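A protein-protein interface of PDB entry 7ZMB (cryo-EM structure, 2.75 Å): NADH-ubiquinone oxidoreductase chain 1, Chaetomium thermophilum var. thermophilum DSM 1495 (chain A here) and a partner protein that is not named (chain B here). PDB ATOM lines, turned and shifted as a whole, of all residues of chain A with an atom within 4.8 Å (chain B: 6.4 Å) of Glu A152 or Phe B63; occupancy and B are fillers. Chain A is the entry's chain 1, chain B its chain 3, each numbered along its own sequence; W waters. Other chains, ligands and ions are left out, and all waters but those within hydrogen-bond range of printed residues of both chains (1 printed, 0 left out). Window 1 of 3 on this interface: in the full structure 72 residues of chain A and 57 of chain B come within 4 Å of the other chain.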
ATOM      1  N   SER A 119       2.045 -19.648  10.613  1.00  0.00           N
ATOM      2  CA  SER A 119       2.578 -18.295  10.892  1.00  0.00           C
ATOM      3  C   SER A 119       3.244 -18.271  12.266  1.00  0.00           C
ATOM      4  O   SER A 119       4.235 -17.544  12.428  1.00  0.00           O
ATOM      5  CB  SER A 119       1.507 -17.250  10.769  1.00  0.00           C
ATOM      6  OG  SER A 119       0.463 -17.488  11.697  1.00  0.00           O
ATOM      7  N   LEU A 148       8.563 -14.296   5.016  1.00  0.00           N
ATOM      8  CA  LEU A 148       7.122 -14.420   5.398  1.00  0.00           C
ATOM      9  C   LEU A 148       6.363 -13.173   4.936  1.00  0.00           C
ATOM     10  O   LEU A 148       5.176 -13.300   4.615  1.00  0.00           O
ATOM     11  CB  LEU A 148       6.963 -14.690   6.900  1.00  0.00           C
ATOM     12  CG  LEU A 148       7.150 -13.516   7.861  1.00  0.00           C
ATOM     13  CD1 LEU A 148       5.816 -12.865   8.199  1.00  0.00           C
ATOM     14  CD2 LEU A 148       7.827 -13.985   9.138  1.00  0.00           C
ATOM     15  N   ILE A 149       7.034 -12.025   4.855  1.00  0.00           N
ATOM     16  CA  ILE A 149       6.403 -10.793   4.304  1.00  0.00           C
ATOM     17  C   ILE A 149       6.227 -11.035   2.796  1.00  0.00           C
ATOM     18  O   ILE A 149       5.492 -10.278   2.150  1.00  0.00           O
ATOM     19  CB  ILE A 149       7.281  -9.559   4.628  1.00  0.00           C
ATOM     20  CG1 ILE A 149       7.436  -9.327   6.129  1.00  0.00           C
ATOM     21  CG2 ILE A 149       6.783  -8.299   3.939  1.00  0.00           C
ATOM     22  CD1 ILE A 149       8.520  -8.329   6.464  1.00  0.00           C
ATOM     23  N   SER A 150       6.879 -12.064   2.255  1.00  0.00           N
ATOM     24  CA  SER A 150       6.787 -12.385   0.807  1.00  0.00           C
ATOM     25  C   SER A 150       5.705 -13.421   0.478  1.00  0.00           C
ATOM     26  O   SER A 150       4.898 -13.139  -0.417  1.00  0.00           O
ATOM     27  CB  SER A 150       8.118 -12.852   0.285  1.00  0.00           C
ATOM     28  OG  SER A 150       9.124 -11.879   0.501  1.00  0.00           O
ATOM     29  N   TYR A 151       5.687 -14.567   1.162  1.00  0.00           N
ATOM     30  CA  TYR A 151       4.783 -15.686   0.773  1.00  0.00           C
ATOM     31  C   TYR A 151       3.442 -15.747   1.515  1.00  0.00           C
ATOM     32  O   TYR A 151       2.555 -16.451   1.013  1.00  0.00           O
ATOM     33  CB  TYR A 151       5.541 -17.006   0.934  1.00  0.00           C
ATOM     34  CG  TYR A 151       5.946 -17.346   2.347  1.00  0.00           C
ATOM     35  CD1 TYR A 151       5.006 -17.629   3.324  1.00  0.00           C
ATOM     36  CD2 TYR A 151       7.278 -17.417   2.707  1.00  0.00           C
ATOM     37  CE1 TYR A 151       5.370 -17.923   4.624  1.00  0.00           C
ATOM     38  CE2 TYR A 151       7.663 -17.726   4.000  1.00  0.00           C
ATOM     39  CZ  TYR A 151       6.706 -17.984   4.962  1.00  0.00           C
ATOM     40  OH  TYR A 151       7.076 -18.291   6.238  1.00  0.00           O
ATOM     41  N   GLU A 152       3.293 -15.094   2.669  1.00  0.00           N
ATOM     42  CA  GLU A 152       2.061 -15.284   3.491  1.00  0.00           C
ATOM     43  C   GLU A 152       0.830 -14.726   2.783  1.00  0.00           C
ATOM     44  O   GLU A 152      -0.178 -15.445   2.692  1.00  0.00           O
ATOM     45  CB  GLU A 152       2.234 -14.658   4.875  1.00  0.00           C
ATOM     46  CG  GLU A 152       1.396 -15.310   5.953  1.00  0.00           C
ATOM     47  CD  GLU A 152       0.619 -14.324   6.805  1.00  0.00           C
ATOM     48  OE1 GLU A 152       0.331 -13.224   6.307  1.00  0.00           O
ATOM     49  OE2 GLU A 152       0.307 -14.660   7.965  1.00  0.00           O
ATOM     50  N   LEU A 153       0.950 -13.519   2.240  1.00  0.00           N
ATOM     51  CA  LEU A 153      -0.182 -12.922   1.504  1.00  0.00           C
ATOM     52  C   LEU A 153      -0.452 -13.797   0.295  1.00  0.00           C
ATOM     53  O   LEU A 153      -1.625 -13.945  -0.061  1.00  0.00           O
ATOM     54  CB  LEU A 153       0.175 -11.495   1.084  1.00  0.00           C
ATOM     55  CG  LEU A 153      -0.451 -10.370   1.901  1.00  0.00           C
ATOM     56  CD1 LEU A 153      -0.285 -10.615   3.389  1.00  0.00           C
ATOM     57  CD2 LEU A 153       0.162  -9.041   1.513  1.00  0.00           C
ATOM     58  N   VAL A 154       0.607 -14.330  -0.319  1.00  0.00           N
ATOM     59  CA  VAL A 154       0.462 -15.125  -1.571  1.00  0.00           C
ATOM     60  C   VAL A 154      -0.384 -16.366  -1.315  1.00  0.00           C
ATOM     61  O   VAL A 154      -1.331 -16.573  -2.083  1.00  0.00           O
ATOM     62  CB  VAL A 154       1.843 -15.460  -2.174  1.00  0.00           C
ATOM     63  CG1 VAL A 154       1.759 -16.585  -3.194  1.00  0.00           C
ATOM     64  CG2 VAL A 154       2.495 -14.231  -2.785  1.00  0.00           C
ATOM     65  N   LEU A 155      -0.105 -17.099  -0.238  1.00  0.00           N
ATOM     66  CA  LEU A 155      -0.890 -18.310   0.115  1.00  0.00           C
ATOM     67  C   LEU A 155      -2.307 -17.919   0.500  1.00  0.00           C
ATOM     68  O   LEU A 155      -3.236 -18.515  -0.046  1.00  0.00           O
ATOM     69  CB  LEU A 155      -0.211 -18.993   1.300  1.00  0.00           C
ATOM     70  CG  LEU A 155       1.133 -19.664   1.032  1.00  0.00           C
ATOM     71  CD1 LEU A 155       1.383 -20.715   2.090  1.00  0.00           C
ATOM     72  CD2 LEU A 155       1.175 -20.302  -0.348  1.00  0.00           C
ATOM     73  N   SER A 156      -2.456 -16.895   1.344  1.00  0.00           N
ATOM     74  CA  SER A 156      -3.782 -16.460   1.844  1.00  0.00           C
ATOM     75  C   SER A 156      -4.631 -15.979   0.675  1.00  0.00           C
ATOM     76  O   SER A 156      -5.829 -16.255   0.687  1.00  0.00           O
ATOM     77  CB  SER A 156      -3.611 -15.406   2.897  1.00  0.00           C
ATOM     78  OG  SER A 156      -3.297 -14.150   2.320  1.00  0.00           O
ATOM     79  N   TRP A 347       5.705  -9.589  -4.810  1.00  0.00           N
ATOM     80  CA  TRP A 347       5.002  -8.340  -4.588  1.00  0.00           C
ATOM     81  C   TRP A 347       4.700  -7.577  -5.870  1.00  0.00           C
ATOM     82  O   TRP A 347       3.799  -6.735  -5.866  1.00  0.00           O
ATOM     83  CB  TRP A 347       5.833  -7.480  -3.634  1.00  0.00           C
ATOM     84  CG  TRP A 347       5.467  -7.690  -2.213  1.00  0.00           C
ATOM     85  CD1 TRP A 347       6.191  -8.355  -1.274  1.00  0.00           C
ATOM     86  CD2 TRP A 347       4.334  -7.160  -1.538  1.00  0.00           C
ATOM     87  NE1 TRP A 347       5.556  -8.316  -0.068  1.00  0.00           N
ATOM     88  CE2 TRP A 347       4.414  -7.578  -0.199  1.00  0.00           C
ATOM     89  CE3 TRP A 347       3.251  -6.382  -1.938  1.00  0.00           C
ATOM     90  CZ2 TRP A 347       3.457  -7.249   0.739  1.00  0.00           C
ATOM     91  CZ3 TRP A 347       2.303  -6.054  -1.007  1.00  0.00           C
ATOM     92  CH2 TRP A 347       2.407  -6.490   0.320  1.00  0.00           C
ATOM     93  N   ILE B  58       9.538  -1.126   4.464  1.00  0.00           N
ATOM     94  CA  ILE B  58       8.353  -0.597   3.806  1.00  0.00           C
ATOM     95  C   ILE B  58       7.459  -1.735   3.322  1.00  0.00           C
ATOM     96  O   ILE B  58       6.230  -1.607   3.299  1.00  0.00           O
ATOM     97  CB  ILE B  58       8.773   0.358   2.672  1.00  0.00           C
ATOM     98  CG1 ILE B  58       9.114   1.725   3.246  1.00  0.00           C
ATOM     99  CG2 ILE B  58       7.699   0.479   1.627  1.00  0.00           C
ATOM    100  CD1 ILE B  58       9.869   2.616   2.311  1.00  0.00           C
ATOM    101  N   TYR B  59       8.054  -2.867   2.954  1.00  0.00           N
ATOM    102  CA  TYR B  59       7.288  -4.088   2.742  1.00  0.00           C
ATOM    103  C   TYR B  59       6.527  -4.514   3.990  1.00  0.00           C
ATOM    104  O   TYR B  59       5.372  -4.928   3.885  1.00  0.00           O
ATOM    105  CB  TYR B  59       8.211  -5.227   2.328  1.00  0.00           C
ATOM    106  CG  TYR B  59       8.633  -5.232   0.890  1.00  0.00           C
ATOM    107  CD1 TYR B  59       9.760  -4.547   0.473  1.00  0.00           C
ATOM    108  CD2 TYR B  59       7.932  -5.951  -0.045  1.00  0.00           C
ATOM    109  CE1 TYR B  59      10.150  -4.565  -0.841  1.00  0.00           C
ATOM    110  CE2 TYR B  59       8.321  -5.977  -1.359  1.00  0.00           C
ATOM    111  CZ  TYR B  59       9.427  -5.286  -1.752  1.00  0.00           C
ATOM    112  OH  TYR B  59       9.800  -5.320  -3.067  1.00  0.00           O
ATOM    113  N   GLY B  60       7.158  -4.443   5.164  1.00  0.00           N
ATOM    114  CA  GLY B  60       6.487  -4.852   6.384  1.00  0.00           C
ATOM    115  C   GLY B  60       5.290  -4.003   6.734  1.00  0.00           C
ATOM    116  O   GLY B  60       4.311  -4.512   7.286  1.00  0.00           O
ATOM    117  N   LEU B  61       5.349  -2.705   6.430  1.00  0.00           N
ATOM    118  CA  LEU B  61       4.210  -1.828   6.669  1.00  0.00           C
ATOM    119  C   LEU B  61       3.055  -2.158   5.733  1.00  0.00           C
ATOM    120  O   LEU B  61       1.904  -2.260   6.170  1.00  0.00           O
ATOM    121  CB  LEU B  61       4.635  -0.364   6.512  1.00  0.00           C
ATOM    122  CG  LEU B  61       5.546   0.235   7.584  1.00  0.00           C
ATOM    123  CD1 LEU B  61       6.212   1.512   7.113  1.00  0.00           C
ATOM    124  CD2 LEU B  61       4.772   0.496   8.849  1.00  0.00           C
ATOM    125  N   VAL B  62       3.335  -2.328   4.439  1.00  0.00           N
ATOM    126  CA  VAL B  62       2.267  -2.644   3.493  1.00  0.00           C
ATOM    127  C   VAL B  62       1.762  -4.067   3.685  1.00  0.00           C
ATOM    128  O   VAL B  62       0.576  -4.337   3.477  1.00  0.00           O
ATOM    129  CB  VAL B  62       2.710  -2.382   2.040  1.00  0.00           C
ATOM    130  CG1 VAL B  62       3.322  -1.023   1.914  1.00  0.00           C
ATOM    131  CG2 VAL B  62       3.696  -3.428   1.573  1.00  0.00           C
ATOM    132  N   PHE B  63       2.637  -4.997   4.079  1.00  0.00           N
ATOM    133  CA  PHE B  63       2.186  -6.344   4.411  1.00  0.00           C
ATOM    134  C   PHE B  63       1.171  -6.325   5.540  1.00  0.00           C
ATOM    135  O   PHE B  63       0.241  -7.136   5.554  1.00  0.00           O
ATOM    136  CB  PHE B  63       3.375  -7.219   4.801  1.00  0.00           C
ATOM    137  CG  PHE B  63       3.021  -8.323   5.745  1.00  0.00           C
ATOM    138  CD1 PHE B  63       2.418  -9.468   5.284  1.00  0.00           C
ATOM    139  CD2 PHE B  63       3.255  -8.199   7.094  1.00  0.00           C
ATOM    140  CE1 PHE B  63       2.079 -10.467   6.142  1.00  0.00           C
ATOM    141  CE2 PHE B  63       2.911  -9.199   7.956  1.00  0.00           C
ATOM    142  CZ  PHE B  63       2.322 -10.339   7.479  1.00  0.00           C
ATOM    143  N   LEU B  64       1.334  -5.409   6.490  1.00  0.00           N
ATOM    144  CA  LEU B  64       0.427  -5.303   7.625  1.00  0.00           C
ATOM    145  C   LEU B  64      -0.999  -5.034   7.166  1.00  0.00           C
ATOM    146  O   LEU B  64      -1.943  -5.654   7.664  1.00  0.00           O
ATOM    147  CB  LEU B  64       0.897  -4.183   8.550  1.00  0.00           C
ATOM    148  CG  LEU B  64       1.866  -4.436   9.699  1.00  0.00           C
ATOM    149  CD1 LEU B  64       2.459  -3.121  10.121  1.00  0.00           C
ATOM    150  CD2 LEU B  64       1.205  -5.093  10.871  1.00  0.00           C
ATOM    151  N   LEU B  65      -1.158  -4.086   6.241  1.00  0.00           N
ATOM    152  CA  LEU B  65      -2.508  -3.653   5.797  1.00  0.00           C
ATOM    153  C   LEU B  65      -3.117  -4.574   4.736  1.00  0.00           C
ATOM    154  O   LEU B  65      -4.349  -4.660   4.712  1.00  0.00           O
ATOM    155  CB  LEU B  65      -2.378  -2.226   5.269  1.00  0.00           C
ATOM    156  CG  LEU B  65      -1.641  -1.260   6.193  1.00  0.00           C
ATOM    157  CD1 LEU B  65      -1.018  -0.121   5.407  1.00  0.00           C
ATOM    158  CD2 LEU B  65      -2.564  -0.734   7.280  1.00  0.00           C
ATOM    159  N   LEU B  66      -2.323  -5.263   3.915  1.00  0.00           N
ATOM    160  CA  LEU B  66      -2.957  -6.072   2.841  1.00  0.00           C
ATOM    161  C   LEU B  66      -3.440  -7.367   3.483  1.00  0.00           C
ATOM    162  O   LEU B  66      -4.347  -7.989   2.921  1.00  0.00           O
ATOM    163  CB  LEU B  66      -1.982  -6.293   1.684  1.00  0.00           C
ATOM    164  CG  LEU B  66      -2.059  -5.254   0.566  1.00  0.00           C
ATOM    165  CD1 LEU B  66      -0.907  -5.404  -0.403  1.00  0.00           C
ATOM    166  CD2 LEU B  66      -3.373  -5.364  -0.182  1.00  0.00           C
ATOM    167  N   ASP B  67      -2.870  -7.735   4.627  1.00  0.00           N
ATOM    168  CA  ASP B  67      -3.379  -8.892   5.404  1.00  0.00           C
ATOM    169  C   ASP B  67      -4.788  -8.560   5.906  1.00  0.00           C
ATOM    170  O   ASP B  67      -5.655  -9.428   5.815  1.00  0.00           O
ATOM    171  CB  ASP B  67      -2.450  -9.153   6.588  1.00  0.00           C
ATOM    172  CG  ASP B  67      -2.507 -10.550   7.177  1.00  0.00           C
ATOM    173  OD1 ASP B  67      -3.401 -11.322   6.787  1.00  0.00           O
ATOM    174  OD2 ASP B  67      -1.644 -10.857   8.024  1.00  0.00           O
ATOM    175  N   LEU B  68      -4.986  -7.356   6.436  1.00  0.00           N
ATOM    176  CA  LEU B  68      -6.315  -6.929   6.939  1.00  0.00           C
ATOM    177  C   LEU B  68      -7.294  -6.965   5.768  1.00  0.00           C
ATOM    178  O   LEU B  68      -8.437  -7.413   5.968  1.00  0.00           O
ATOM    179  CB  LEU B  68      -6.179  -5.514   7.495  1.00  0.00           C
ATOM    180  CG  LEU B  68      -5.199  -5.353   8.656  1.00  0.00           C
ATOM    181  CD1 LEU B  68      -4.895  -3.888   8.914  1.00  0.00           C
ATOM    182  CD2 LEU B  68      -5.729  -6.017   9.914  1.00  0.00           C
HETATM  183  O   HOH W   1      -2.060 -12.879   4.893  1.00  0.00           O
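Among the printed residues, merely in contact across the chains: Trp A347 with Tyr B59 (3.2 Å), Glu A152 with Phe B63 (3.3 Å), Trp A347 with Leu B66 (3.3 Å), Leu A153 with Leu B66 (3.5 Å), Leu A153 with Phe B63 (3.5 Å), Glu A152 with Asp B67 (3.5 Å), Trp A347 with Val B62 (3.6 Å), Ile A149 with Tyr B59 (3.7 Å), Ile A149 with Phe B63 (3.7 Å) and Trp A347 with Phe B63 (3.99 Å).
Water W1 lies within hydrogen-bond range of OD1 of Asp B67, OE1 of Glu A152 and OG of Ser A156.
Of the 11 printed residues of chain A, 4 touch a printed residue of chain B.
Hydrophobic or aromatic side chains of chain A within 4 Å of the printed part of chain B: Ile A149, Leu A153 and Trp A347.
Among the printed residues, no Asp or Glu carboxylate lies within 4 Å of a Lys or Arg side-chain nitrogen of the other chain.
NE1 of Trp A347 lies within hydrogen-bond range of O of Ile A149, at 3.0 Å.
The backbone carbonyl oxygen (O) of Glu A152 sits at hydrogen-bond distance from the side-chain hydroxyl (OG) of Ser A156 (3.4 Å).
O of Leu A153 lies within hydrogen-bond range of OG of Ser A156 (2.9 Å).
Of the printed residues of chain B, Ile A149 touches Tyr B59 (3.7 Å) and Phe B63 (3.7 Å).
Of chain B, only Phe B63 and Asp B67 come within 4 Å of Glu A152.
Of the printed residues of chain B, Trp A347 touches Tyr B59 (3.2 Å), Val B62 (3.6 Å), Phe B63 (3.99 Å) and Leu B66 (3.3 Å).
Printed residues of chain A within 4 Å of Phe B63: Ile A149 (3.7 Å), Glu A152 (3.3 Å), Leu A153 (3.5 Å) and Trp A347 (3.99 Å).
The nearest printed residue of chain B that does not touch Glu A152 is Leu B66 (7.5 Å).
The nearest printed residue of chain A that does not touch Phe B63 is Leu A148 (4.4 Å).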
